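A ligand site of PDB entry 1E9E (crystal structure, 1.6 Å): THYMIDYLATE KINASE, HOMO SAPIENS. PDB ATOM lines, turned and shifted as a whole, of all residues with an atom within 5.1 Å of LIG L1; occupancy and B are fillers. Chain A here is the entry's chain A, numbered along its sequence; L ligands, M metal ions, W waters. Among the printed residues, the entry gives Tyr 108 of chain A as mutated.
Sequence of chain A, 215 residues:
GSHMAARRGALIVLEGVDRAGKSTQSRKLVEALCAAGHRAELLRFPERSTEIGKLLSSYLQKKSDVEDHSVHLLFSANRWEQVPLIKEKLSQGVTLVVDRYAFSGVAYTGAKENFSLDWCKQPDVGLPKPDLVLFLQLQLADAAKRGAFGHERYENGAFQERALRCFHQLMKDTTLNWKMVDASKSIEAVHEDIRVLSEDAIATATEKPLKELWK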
ATOM      1  N   LYS A  22     -11.708  -3.509  18.244  1.00  0.00           N
ATOM      2  CA  LYS A  22     -10.996  -3.642  19.509  1.00  0.00           C
ATOM      3  C   LYS A  22     -10.815  -5.051  20.007  1.00  0.00           C
ATOM      4  O   LYS A  22      -9.743  -5.461  20.474  1.00  0.00           O
ATOM      5  CB  LYS A  22     -11.785  -2.826  20.563  1.00  0.00           C
ATOM      6  CG  LYS A  22     -11.821  -1.351  20.208  1.00  0.00           C
ATOM      7  CD  LYS A  22     -12.550  -0.527  21.248  1.00  0.00           C
ATOM      8  CE  LYS A  22     -13.961  -1.012  21.538  1.00  0.00           C
ATOM      9  NZ  LYS A  22     -14.840  -0.843  20.339  1.00  0.00           N
ATOM     10  N   SER A  23     -11.941  -5.786  20.052  1.00  0.00           N
ATOM     11  CA  SER A  23     -11.833  -7.144  20.610  1.00  0.00           C
ATOM     12  C   SER A  23     -10.992  -8.041  19.732  1.00  0.00           C
ATOM     13  O   SER A  23     -10.137  -8.782  20.241  1.00  0.00           O
ATOM     14  CB  SER A  23     -13.222  -7.711  20.912  1.00  0.00           C
ATOM     15  OG  SER A  23     -13.889  -6.770  21.754  1.00  0.00           O
ATOM     16  N   PHE A  45     -12.981  -4.220  29.651  1.00  0.00           N
ATOM     17  CA  PHE A  45     -13.954  -3.495  30.444  1.00  0.00           C
ATOM     18  C   PHE A  45     -15.132  -3.176  29.538  1.00  0.00           C
ATOM     19  O   PHE A  45     -14.917  -2.813  28.392  1.00  0.00           O
ATOM     20  CB  PHE A  45     -13.352  -2.211  31.083  1.00  0.00           C
ATOM     21  CG  PHE A  45     -12.325  -2.632  32.118  1.00  0.00           C
ATOM     22  CD1 PHE A  45     -12.754  -3.150  33.327  1.00  0.00           C
ATOM     23  CD2 PHE A  45     -10.970  -2.524  31.838  1.00  0.00           C
ATOM     24  CE1 PHE A  45     -11.815  -3.549  34.272  1.00  0.00           C
ATOM     25  CE2 PHE A  45     -10.043  -2.948  32.785  1.00  0.00           C
ATOM     26  CZ  PHE A  45     -10.455  -3.434  34.011  1.00  0.00           C
ATOM     27  N   PRO A  46     -16.375  -3.381  29.989  1.00  0.00           N
ATOM     28  CA  PRO A  46     -16.655  -3.877  31.310  1.00  0.00           C
ATOM     29  C   PRO A  46     -16.263  -5.328  31.502  1.00  0.00           C
ATOM     30  O   PRO A  46     -16.338  -6.152  30.571  1.00  0.00           O
ATOM     31  CB  PRO A  46     -18.187  -3.767  31.422  1.00  0.00           C
ATOM     32  CG  PRO A  46     -18.647  -3.827  29.989  1.00  0.00           C
ATOM     33  CD  PRO A  46     -17.598  -3.083  29.209  1.00  0.00           C
ATOM     34  N   ARG A  48     -17.568  -8.261  32.782  1.00  0.00           N
ATOM     35  CA  ARG A  48     -18.934  -8.656  33.096  1.00  0.00           C
ATOM     36  C   ARG A  48     -19.123  -9.807  34.063  1.00  0.00           C
ATOM     37  O   ARG A  48     -20.283 -10.101  34.356  1.00  0.00           O
ATOM     38  CB  ARG A  48     -19.667  -8.986  31.792  1.00  0.00           C
ATOM     39  CG  ARG A  48     -19.722  -7.787  30.849  1.00  0.00           C
ATOM     40  CD  ARG A  48     -20.490  -8.191  29.594  1.00  0.00           C
ATOM     41  NE  ARG A  48     -20.365  -7.189  28.559  1.00  0.00           N
ATOM     42  CZ  ARG A  48     -21.412  -6.811  27.812  1.00  0.00           C
ATOM     43  NH1 ARG A  48     -22.623  -7.293  28.038  1.00  0.00           N
ATOM     44  NH2 ARG A  48     -21.254  -5.923  26.847  1.00  0.00           N
ATOM     45  N   LEU A  60     -26.683  -3.057  29.806  1.00  0.00           N
ATOM     46  CA  LEU A  60     -26.333  -2.997  28.387  1.00  0.00           C
ATOM     47  C   LEU A  60     -27.257  -3.856  27.537  1.00  0.00           C
ATOM     48  O   LEU A  60     -27.558  -3.458  26.401  1.00  0.00           O
ATOM     49  CB  LEU A  60     -24.880  -3.422  28.225  1.00  0.00           C
ATOM     50  CG  LEU A  60     -23.848  -2.417  28.761  1.00  0.00           C
ATOM     51  CD1 LEU A  60     -22.453  -3.022  28.667  1.00  0.00           C
ATOM     52  CD2 LEU A  60     -23.925  -1.092  28.020  1.00  0.00           C
ATOM     53  N   PHE A  75     -19.479   1.536  36.108  1.00  0.00           N
ATOM     54  CA  PHE A  75     -18.448   1.252  35.083  1.00  0.00           C
ATOM     55  C   PHE A  75     -17.071   1.551  35.663  1.00  0.00           C
ATOM     56  O   PHE A  75     -16.132   0.814  35.411  1.00  0.00           O
ATOM     57  CB  PHE A  75     -18.712   2.041  33.817  1.00  0.00           C
ATOM     58  CG  PHE A  75     -19.589   1.419  32.779  1.00  0.00           C
ATOM     59  CD1 PHE A  75     -19.205   0.238  32.152  1.00  0.00           C
ATOM     60  CD2 PHE A  75     -20.790   2.007  32.402  1.00  0.00           C
ATOM     61  CE1 PHE A  75     -19.998  -0.334  31.172  1.00  0.00           C
ATOM     62  CE2 PHE A  75     -21.585   1.450  31.402  1.00  0.00           C
ATOM     63  CZ  PHE A  75     -21.180   0.269  30.799  1.00  0.00           C
ATOM     64  N   ARG A  79     -13.680  -1.024  37.026  1.00  0.00           N
ATOM     65  CA  ARG A  79     -12.266  -0.913  36.753  1.00  0.00           C
ATOM     66  C   ARG A  79     -11.489  -0.979  38.075  1.00  0.00           C
ATOM     67  O   ARG A  79     -10.533  -1.728  38.199  1.00  0.00           O
ATOM     68  CB  ARG A  79     -11.849   0.349  36.008  1.00  0.00           C
ATOM     69  CG  ARG A  79     -12.126   0.205  34.507  1.00  0.00           C
ATOM     70  CD  ARG A  79     -11.986   1.511  33.812  1.00  0.00           C
ATOM     71  NE  ARG A  79     -12.879   2.639  34.072  1.00  0.00           N
ATOM     72  CZ  ARG A  79     -14.079   2.719  33.475  1.00  0.00           C
ATOM     73  NH1 ARG A  79     -14.531   1.758  32.669  1.00  0.00           N
ATOM     74  NH2 ARG A  79     -14.820   3.816  33.632  1.00  0.00           N
ATOM     75  N   ASP A  99      -9.119  -4.315  26.503  1.00  0.00           N
ATOM     76  CA  ASP A  99     -10.146  -3.938  25.516  1.00  0.00           C
ATOM     77  C   ASP A  99     -11.089  -2.958  26.208  1.00  0.00           C
ATOM     78  O   ASP A  99     -11.942  -3.445  26.968  1.00  0.00           O
ATOM     79  CB  ASP A  99     -10.842  -5.244  25.135  1.00  0.00           C
ATOM     80  CG  ASP A  99     -11.929  -5.199  24.100  1.00  0.00           C
ATOM     81  OD1 ASP A  99     -12.290  -4.092  23.653  1.00  0.00           O
ATOM     82  OD2 ASP A  99     -12.384  -6.321  23.780  1.00  0.00           O
ATOM     83  N   ARG A 100     -10.838  -1.693  26.020  1.00  0.00           N
ATOM     84  CA  ARG A 100     -11.558  -0.575  26.599  1.00  0.00           C
ATOM     85  C   ARG A 100     -11.099  -0.298  28.049  1.00  0.00           C
ATOM     86  O   ARG A 100     -10.680  -1.161  28.777  1.00  0.00           O
ATOM     87  CB  ARG A 100     -13.075  -0.753  26.689  1.00  0.00           C
ATOM     88  CG  ARG A 100     -13.804  -0.850  25.347  1.00  0.00           C
ATOM     89  CD  ARG A 100     -15.303  -0.746  25.652  1.00  0.00           C
ATOM     90  NE  ARG A 100     -16.115  -1.055  24.483  1.00  0.00           N
ATOM     91  CZ  ARG A 100     -16.467  -0.189  23.551  1.00  0.00           C
ATOM     92  NH1 ARG A 100     -16.142   1.094  23.541  1.00  0.00           N
ATOM     93  NH2 ARG A 100     -17.217  -0.635  22.535  1.00  0.00           N
ATOM     94  N   TYR A 101     -11.179   0.985  28.359  1.00  0.00           N
ATOM     95  CA  TYR A 101     -10.814   1.407  29.727  1.00  0.00           C
ATOM     96  C   TYR A 101     -11.602   2.657  30.078  1.00  0.00           C
ATOM     97  O   TYR A 101     -12.764   2.825  29.684  1.00  0.00           O
ATOM     98  CB  TYR A 101      -9.324   1.637  29.787  1.00  0.00           C
ATOM     99  CG  TYR A 101      -8.561   1.625  31.090  1.00  0.00           C
ATOM    100  CD1 TYR A 101      -8.628   0.579  31.973  1.00  0.00           C
ATOM    101  CD2 TYR A 101      -7.723   2.714  31.380  1.00  0.00           C
ATOM    102  CE1 TYR A 101      -7.895   0.546  33.154  1.00  0.00           C
ATOM    103  CE2 TYR A 101      -6.967   2.669  32.549  1.00  0.00           C
ATOM    104  CZ  TYR A 101      -7.063   1.620  33.412  1.00  0.00           C
ATOM    105  OH  TYR A 101      -6.289   1.627  34.559  1.00  0.00           O
ATOM    106  N   SER A 104     -13.378   4.883  27.218  1.00  0.00           N
ATOM    107  CA  SER A 104     -14.732   4.498  26.847  1.00  0.00           C
ATOM    108  C   SER A 104     -15.740   4.933  27.926  1.00  0.00           C
ATOM    109  O   SER A 104     -16.853   5.365  27.632  1.00  0.00           O
ATOM    110  CB  SER A 104     -14.861   2.977  26.685  1.00  0.00           C
ATOM    111  OG  SER A 104     -14.493   2.635  25.327  1.00  0.00           O
ATOM    112  N   GLY A 105     -15.322   4.831  29.191  1.00  0.00           N
ATOM    113  CA  GLY A 105     -16.237   5.228  30.268  1.00  0.00           C
ATOM    114  C   GLY A 105     -16.650   6.676  30.108  1.00  0.00           C
ATOM    115  O   GLY A 105     -17.829   7.013  30.226  1.00  0.00           O
ATOM    116  N   TYR A 108     -18.660   7.321  26.475  1.00  0.00           N
ATOM    117  CA  TYR A 108     -20.039   6.840  26.301  1.00  0.00           C
ATOM    118  C   TYR A 108     -20.986   7.587  27.207  1.00  0.00           C
ATOM    119  O   TYR A 108     -22.084   7.967  26.790  1.00  0.00           O
ATOM    120  CB  TYR A 108     -20.065   5.301  26.411  1.00  0.00           C
ATOM    121  CG  TYR A 108     -19.599   4.750  25.060  1.00  0.00           C
ATOM    122  CD1 TYR A 108     -18.248   4.653  24.787  1.00  0.00           C
ATOM    123  CD2 TYR A 108     -20.535   4.395  24.082  1.00  0.00           C
ATOM    124  CE1 TYR A 108     -17.825   4.159  23.550  1.00  0.00           C
ATOM    125  CE2 TYR A 108     -20.094   3.925  22.852  1.00  0.00           C
ATOM    126  CZ  TYR A 108     -18.751   3.810  22.602  1.00  0.00           C
ATOM    127  OH  TYR A 108     -18.313   3.349  21.374  1.00  0.00           O
ATOM    128  N   THR A 109     -20.601   7.851  28.457  1.00  0.00           N
ATOM    129  CA  THR A 109     -21.522   8.628  29.311  1.00  0.00           C
ATOM    130  C   THR A 109     -21.544  10.068  28.814  1.00  0.00           C
ATOM    131  O   THR A 109     -22.599  10.700  28.850  1.00  0.00           O
ATOM    132  CB  THR A 109     -21.055   8.584  30.782  1.00  0.00           C
ATOM    133  OG1 THR A 109     -21.209   7.230  31.224  1.00  0.00           O
ATOM    134  CG2 THR A 109     -21.854   9.510  31.679  1.00  0.00           C
ATOM    135  N   GLU A 152     -27.547  -4.113  22.004  1.00  0.00           N
ATOM    136  CA  GLU A 152     -27.280  -3.544  23.313  1.00  0.00           C
ATOM    137  C   GLU A 152     -27.498  -2.032  23.273  1.00  0.00           C
ATOM    138  O   GLU A 152     -27.571  -1.384  22.224  1.00  0.00           O
ATOM    139  CB  GLU A 152     -25.846  -3.770  23.800  1.00  0.00           C
ATOM    140  CG  GLU A 152     -25.558  -5.183  24.251  1.00  0.00           C
ATOM    141  CD  GLU A 152     -24.292  -5.407  25.032  1.00  0.00           C
ATOM    142  OE1 GLU A 152     -23.315  -4.622  24.970  1.00  0.00           O
ATOM    143  OE2 GLU A 152     -24.282  -6.436  25.752  1.00  0.00           O
ATOM    144  N   ARG A 153     -27.570  -1.473  24.486  1.00  0.00           N
ATOM    145  CA  ARG A 153     -27.708  -0.023  24.568  1.00  0.00           C
ATOM    146  C   ARG A 153     -26.462   0.566  23.892  1.00  0.00           C
ATOM    147  O   ARG A 153     -25.412  -0.071  23.868  1.00  0.00           O
ATOM    148  CB  ARG A 153     -27.759   0.438  26.034  1.00  0.00           C
ATOM    149  CG  ARG A 153     -29.048   0.109  26.775  1.00  0.00           C
ATOM    150  CD  ARG A 153     -29.001   0.629  28.228  1.00  0.00           C
ATOM    151  NE  ARG A 153     -30.131   0.084  28.980  1.00  0.00           N
ATOM    152  CZ  ARG A 153     -31.371   0.522  28.919  1.00  0.00           C
ATOM    153  NH1 ARG A 153     -31.648   1.545  28.117  1.00  0.00           N
ATOM    154  NH2 ARG A 153     -32.309  -0.066  29.659  1.00  0.00           N
ATOM    155  N   TYR A 154     -26.594   1.766  23.390  1.00  0.00           N
ATOM    156  CA  TYR A 154     -25.568   2.540  22.723  1.00  0.00           C
ATOM    157  C   TYR A 154     -25.276   2.079  21.294  1.00  0.00           C
ATOM    158  O   TYR A 154     -24.511   2.738  20.606  1.00  0.00           O
ATOM    159  CB  TYR A 154     -24.260   2.544  23.526  1.00  0.00           C
ATOM    160  CG  TYR A 154     -24.374   2.980  24.983  1.00  0.00           C
ATOM    161  CD1 TYR A 154     -25.453   3.699  25.470  1.00  0.00           C
ATOM    162  CD2 TYR A 154     -23.363   2.657  25.862  1.00  0.00           C
ATOM    163  CE1 TYR A 154     -25.510   4.086  26.797  1.00  0.00           C
ATOM    164  CE2 TYR A 154     -23.402   3.027  27.191  1.00  0.00           C
ATOM    165  CZ  TYR A 154     -24.486   3.739  27.657  1.00  0.00           C
ATOM    166  OH  TYR A 154     -24.538   4.106  28.980  1.00  0.00           O
ATOM    167  N   GLN A 160     -23.214   6.458  18.827  1.00  0.00           N
ATOM    168  CA  GLN A 160     -21.810   6.269  18.464  1.00  0.00           C
ATOM    169  C   GLN A 160     -21.162   7.558  17.985  1.00  0.00           C
ATOM    170  O   GLN A 160     -20.004   7.823  18.293  1.00  0.00           O
ATOM    171  CB  GLN A 160     -21.651   5.183  17.376  1.00  0.00           C
ATOM    172  CG  GLN A 160     -22.092   3.803  17.841  1.00  0.00           C
ATOM    173  CD  GLN A 160     -21.209   3.290  18.972  1.00  0.00           C
ATOM    174  OE1 GLN A 160     -19.988   3.457  18.922  1.00  0.00           O
ATOM    175  NE2 GLN A 160     -21.840   2.702  19.951  1.00  0.00           N
HETATM  176  P1  LIG L   1     -18.078  -3.672  24.366  1.00  0.00           P
HETATM  177  O1  LIG L   1     -18.453  -3.015  23.043  1.00  0.00           O
HETATM  178  O2  LIG L   1     -16.611  -3.594  24.548  1.00  0.00           O
HETATM  179  O3  LIG L   1     -18.720  -5.080  24.465  1.00  0.00           O
HETATM  180  O4  LIG L   1     -18.696  -2.783  25.519  1.00  0.00           O
HETATM  181  C1  LIG L   1     -20.103  -2.725  25.844  1.00  0.00           C
HETATM  182  C2  LIG L   1     -20.419  -1.229  26.032  1.00  0.00           C
HETATM  183  O5  LIG L   1     -20.037  -0.599  27.254  1.00  0.00           O
HETATM  184  C3  LIG L   1     -20.015  -0.332  24.895  1.00  0.00           C
HETATM  185  O6  LIG L   1     -21.157   0.290  24.353  1.00  0.00           O
HETATM  186  C4  LIG L   1     -19.165   0.764  25.566  1.00  0.00           C
HETATM  187  C5  LIG L   1     -19.701   0.727  26.993  1.00  0.00           C
HETATM  188  N1  LIG L   1     -18.918   1.291  28.086  1.00  0.00           N
HETATM  189  C6  LIG L   1     -19.443   2.356  28.826  1.00  0.00           C
HETATM  190  O7  LIG L   1     -20.476   2.952  28.595  1.00  0.00           O
HETATM  191  N2  LIG L   1     -18.615   2.686  29.880  1.00  0.00           N
HETATM  192  C7  LIG L   1     -17.438   2.029  30.161  1.00  0.00           C
HETATM  193  O8  LIG L   1     -16.678   2.420  31.242  1.00  0.00           O
HETATM  194  C8  LIG L   1     -16.971   0.903  29.306  1.00  0.00           C
HETATM  195  C9  LIG L   1     -15.715   0.203  29.635  1.00  0.00           C
HETATM  196  C10 LIG L   1     -17.800   0.586  28.287  1.00  0.00           C
HETATM  197  P1  LG2 L   2     -15.165  -4.065  18.583  1.00  0.00           P
HETATM  198  O1  LG2 L   2     -14.437  -2.779  18.420  1.00  0.00           O
HETATM  199  O2  LG2 L   2     -14.772  -4.873  19.757  1.00  0.00           O
HETATM  200  O3  LG2 L   2     -16.727  -3.871  18.576  1.00  0.00           O
HETATM  201  P2  LG2 L   2     -14.702  -6.427  16.868  1.00  0.00           P
HETATM  202  O4  LG2 L   2     -15.620  -7.251  17.679  1.00  0.00           O
HETATM  203  O5  LG2 L   2     -13.237  -6.771  16.953  1.00  0.00           O
HETATM  204  O6  LG2 L   2     -14.859  -4.858  17.182  1.00  0.00           O
HETATM  205  O7  LG2 L   2     -15.087  -6.432  15.332  1.00  0.00           O
HETATM  206  C1  LG2 L   2     -16.404  -6.026  14.927  1.00  0.00           C
HETATM  207  C2  LG2 L   2     -16.807  -6.861  13.698  1.00  0.00           C
HETATM  208  O8  LG2 L   2     -16.012  -6.416  12.607  1.00  0.00           O
HETATM  209  C3  LG2 L   2     -16.593  -8.354  13.830  1.00  0.00           C
HETATM  210  O9  LG2 L   2     -17.482  -9.050  12.953  1.00  0.00           O
HETATM  211  C4  LG2 L   2     -15.162  -8.505  13.252  1.00  0.00           C
HETATM  212  O10 LG2 L   2     -14.844  -9.730  12.648  1.00  0.00           O
HETATM  213  C5  LG2 L   2     -15.198  -7.451  12.140  1.00  0.00           C
HETATM  214  N1  LG2 L   2     -13.864  -6.865  11.919  1.00  0.00           N
HETATM  215  C6  LG2 L   2     -12.904  -6.627  12.882  1.00  0.00           C
HETATM  216  N2  LG2 L   2     -11.842  -6.026  12.353  1.00  0.00           N
HETATM  217  C7  LG2 L   2     -12.150  -5.862  10.992  1.00  0.00           C
HETATM  218  C8  LG2 L   2     -11.435  -5.308   9.938  1.00  0.00           C
HETATM  219  N3  LG2 L   2     -10.236  -4.789  10.031  1.00  0.00           N
HETATM  220  N4  LG2 L   2     -12.095  -5.353   8.759  1.00  0.00           N
HETATM  221  C9  LG2 L   2     -13.311  -5.875   8.619  1.00  0.00           C
HETATM  222  N5  LG2 L   2     -14.063  -6.421   9.557  1.00  0.00           N
HETATM  223  C10 LG2 L   2     -13.388  -6.364  10.699  1.00  0.00           C
HETATM  224 MG    MG M   1     -15.605  -5.679  21.380  1.00  0.00          MG
HETATM  225  O   HOH W   1     -17.397  -4.534  21.233  1.00  0.00           O
HETATM  226  O   HOH W   2     -17.556  -2.056  20.193  1.00  0.00           O
HETATM  227  O   HOH W   3     -22.012   4.696  29.842  1.00  0.00           O
HETATM  228  O   HOH W   4     -23.131  -1.519  24.037  1.00  0.00           O
HETATM  229  O   HOH W   5     -20.095   0.832  21.607  1.00  0.00           O
HETATM  230  O   HOH W   6     -16.393  -6.785  23.108  1.00  0.00           O
HETATM  231  O   HOH W   7     -19.190   4.844  31.530  1.00  0.00           O
HETATM  232  O   HOH W   8     -14.777  -4.285  22.637  1.00  0.00           O
HETATM  233  O   HOH W   9     -15.173  -4.860  26.450  1.00  0.00           O
HETATM  234  O   HOH W  10     -20.495  -2.478  21.455  1.00  0.00           O
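The guanidinium group (NE) of Arg 100 is in salt-bridge range of an oxygen (O2) of LIG L1 (2.6 Å). An oxygen (O8) of LIG L1 is in hydrogen-bond range of the guanidinium group (NH1) of Arg 79 (2.7 Å). The backbone NH (N) of Gly 105 lies close to an oxygen (O8) of LIG L1 (3.4 Å). An oxygen (O3) of LIG L1 lies within salt-bridge range of the guanidinium group of Arg 48, 3.6 Å away. The backbone NH of Lys 22 is in hydrogen-bond range of an oxygen (O1) of LG2 L2 (2.8 Å). NZ of Lys 22 is in salt-bridge range of O1 of LG2 L2, at 2.8 Å. N of Ser 23 sits close to O2 of LG2 L2 (3.0 Å).
The side-chain hydroxyl of Ser 104 is in hydrogen-bond range of the guanidinium group of Arg 100 (2.9 Å). NH1 of Arg 79 is in hydrogen-bond range of O of Phe 75. OE1 of Gln 160 sits at hydrogen-bond distance from OH of Tyr 108, 3.0 Å away. NE2 of Gln 160 is in hydrogen-bond range of O of Tyr 154 (2.8 Å). N of Phe 45 lies within hydrogen-bond range of O of Asp 99, 3.0 Å away. NH1 of Arg 48 is in salt-bridge range of OE2 of Glu 152 (3.0 Å). O of Leu 60 sits at hydrogen-bond distance from N of Arg 153 (2.8 Å).
Merely in contact with LIG L1: Phe 45 (3.4 Å), Pro 46 (3.7 Å), Leu 60 (3.7 Å), Phe 75 (3.2 Å), Tyr 101 (3.9 Å), Ser 104 (3.9 Å), Tyr 108 (3.2 Å), Glu 152 (3.8 Å) and Tyr 154 (3.2 Å). Hydrophobic or aromatic side chains within 4 Å of LIG L1: Phe 45, Pro 46, Leu 60, Phe 75, Tyr 108 and Tyr 154. 13 residues have an atom within 4 Å of LIG L1: Phe 45, Pro 46, Arg 48, Leu 60, Phe 75, Arg 79, Arg 100, Tyr 101, Ser 104, Gly 105, Tyr 108, Glu 152 and Tyr 154.
Water W1 lies within hydrogen-bond range of O1 of LIG L1 (2.6 Å) and O3 of LG2 L2 (2.8 Å). Water W3 lies within hydrogen-bond range of O7 of LIG L1 (2.6 Å), OH of Tyr 154 (2.7 Å) and OG1 of Thr 109 (3.0 Å). Water W4 lies within hydrogen-bond range of an oxygen (O6) of LIG L1, the backbone carbonyl oxygen (O) of Arg 153 and the side-chain carboxylate (OE1) of Glu 152. Water W9 lies within hydrogen-bond range of an oxygen (O2) of LIG L1 (2.7 Å) and the backbone carbonyl oxygen of Phe 45 (2.8 Å). Water W8 lies within hydrogen-bond range of the side-chain carboxylate (OD1) of Asp 99 (2.7 Å) and an oxygen (O2) of LIG L1 (2.7 Å). Water W2 lies within hydrogen-bond range of O3 of LG2 L2 (2.6 Å), NH2 of Arg 100 (2.8 Å), NZ of Lys 22 (3.0 Å) and O1 of LIG L1 (3.1 Å).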
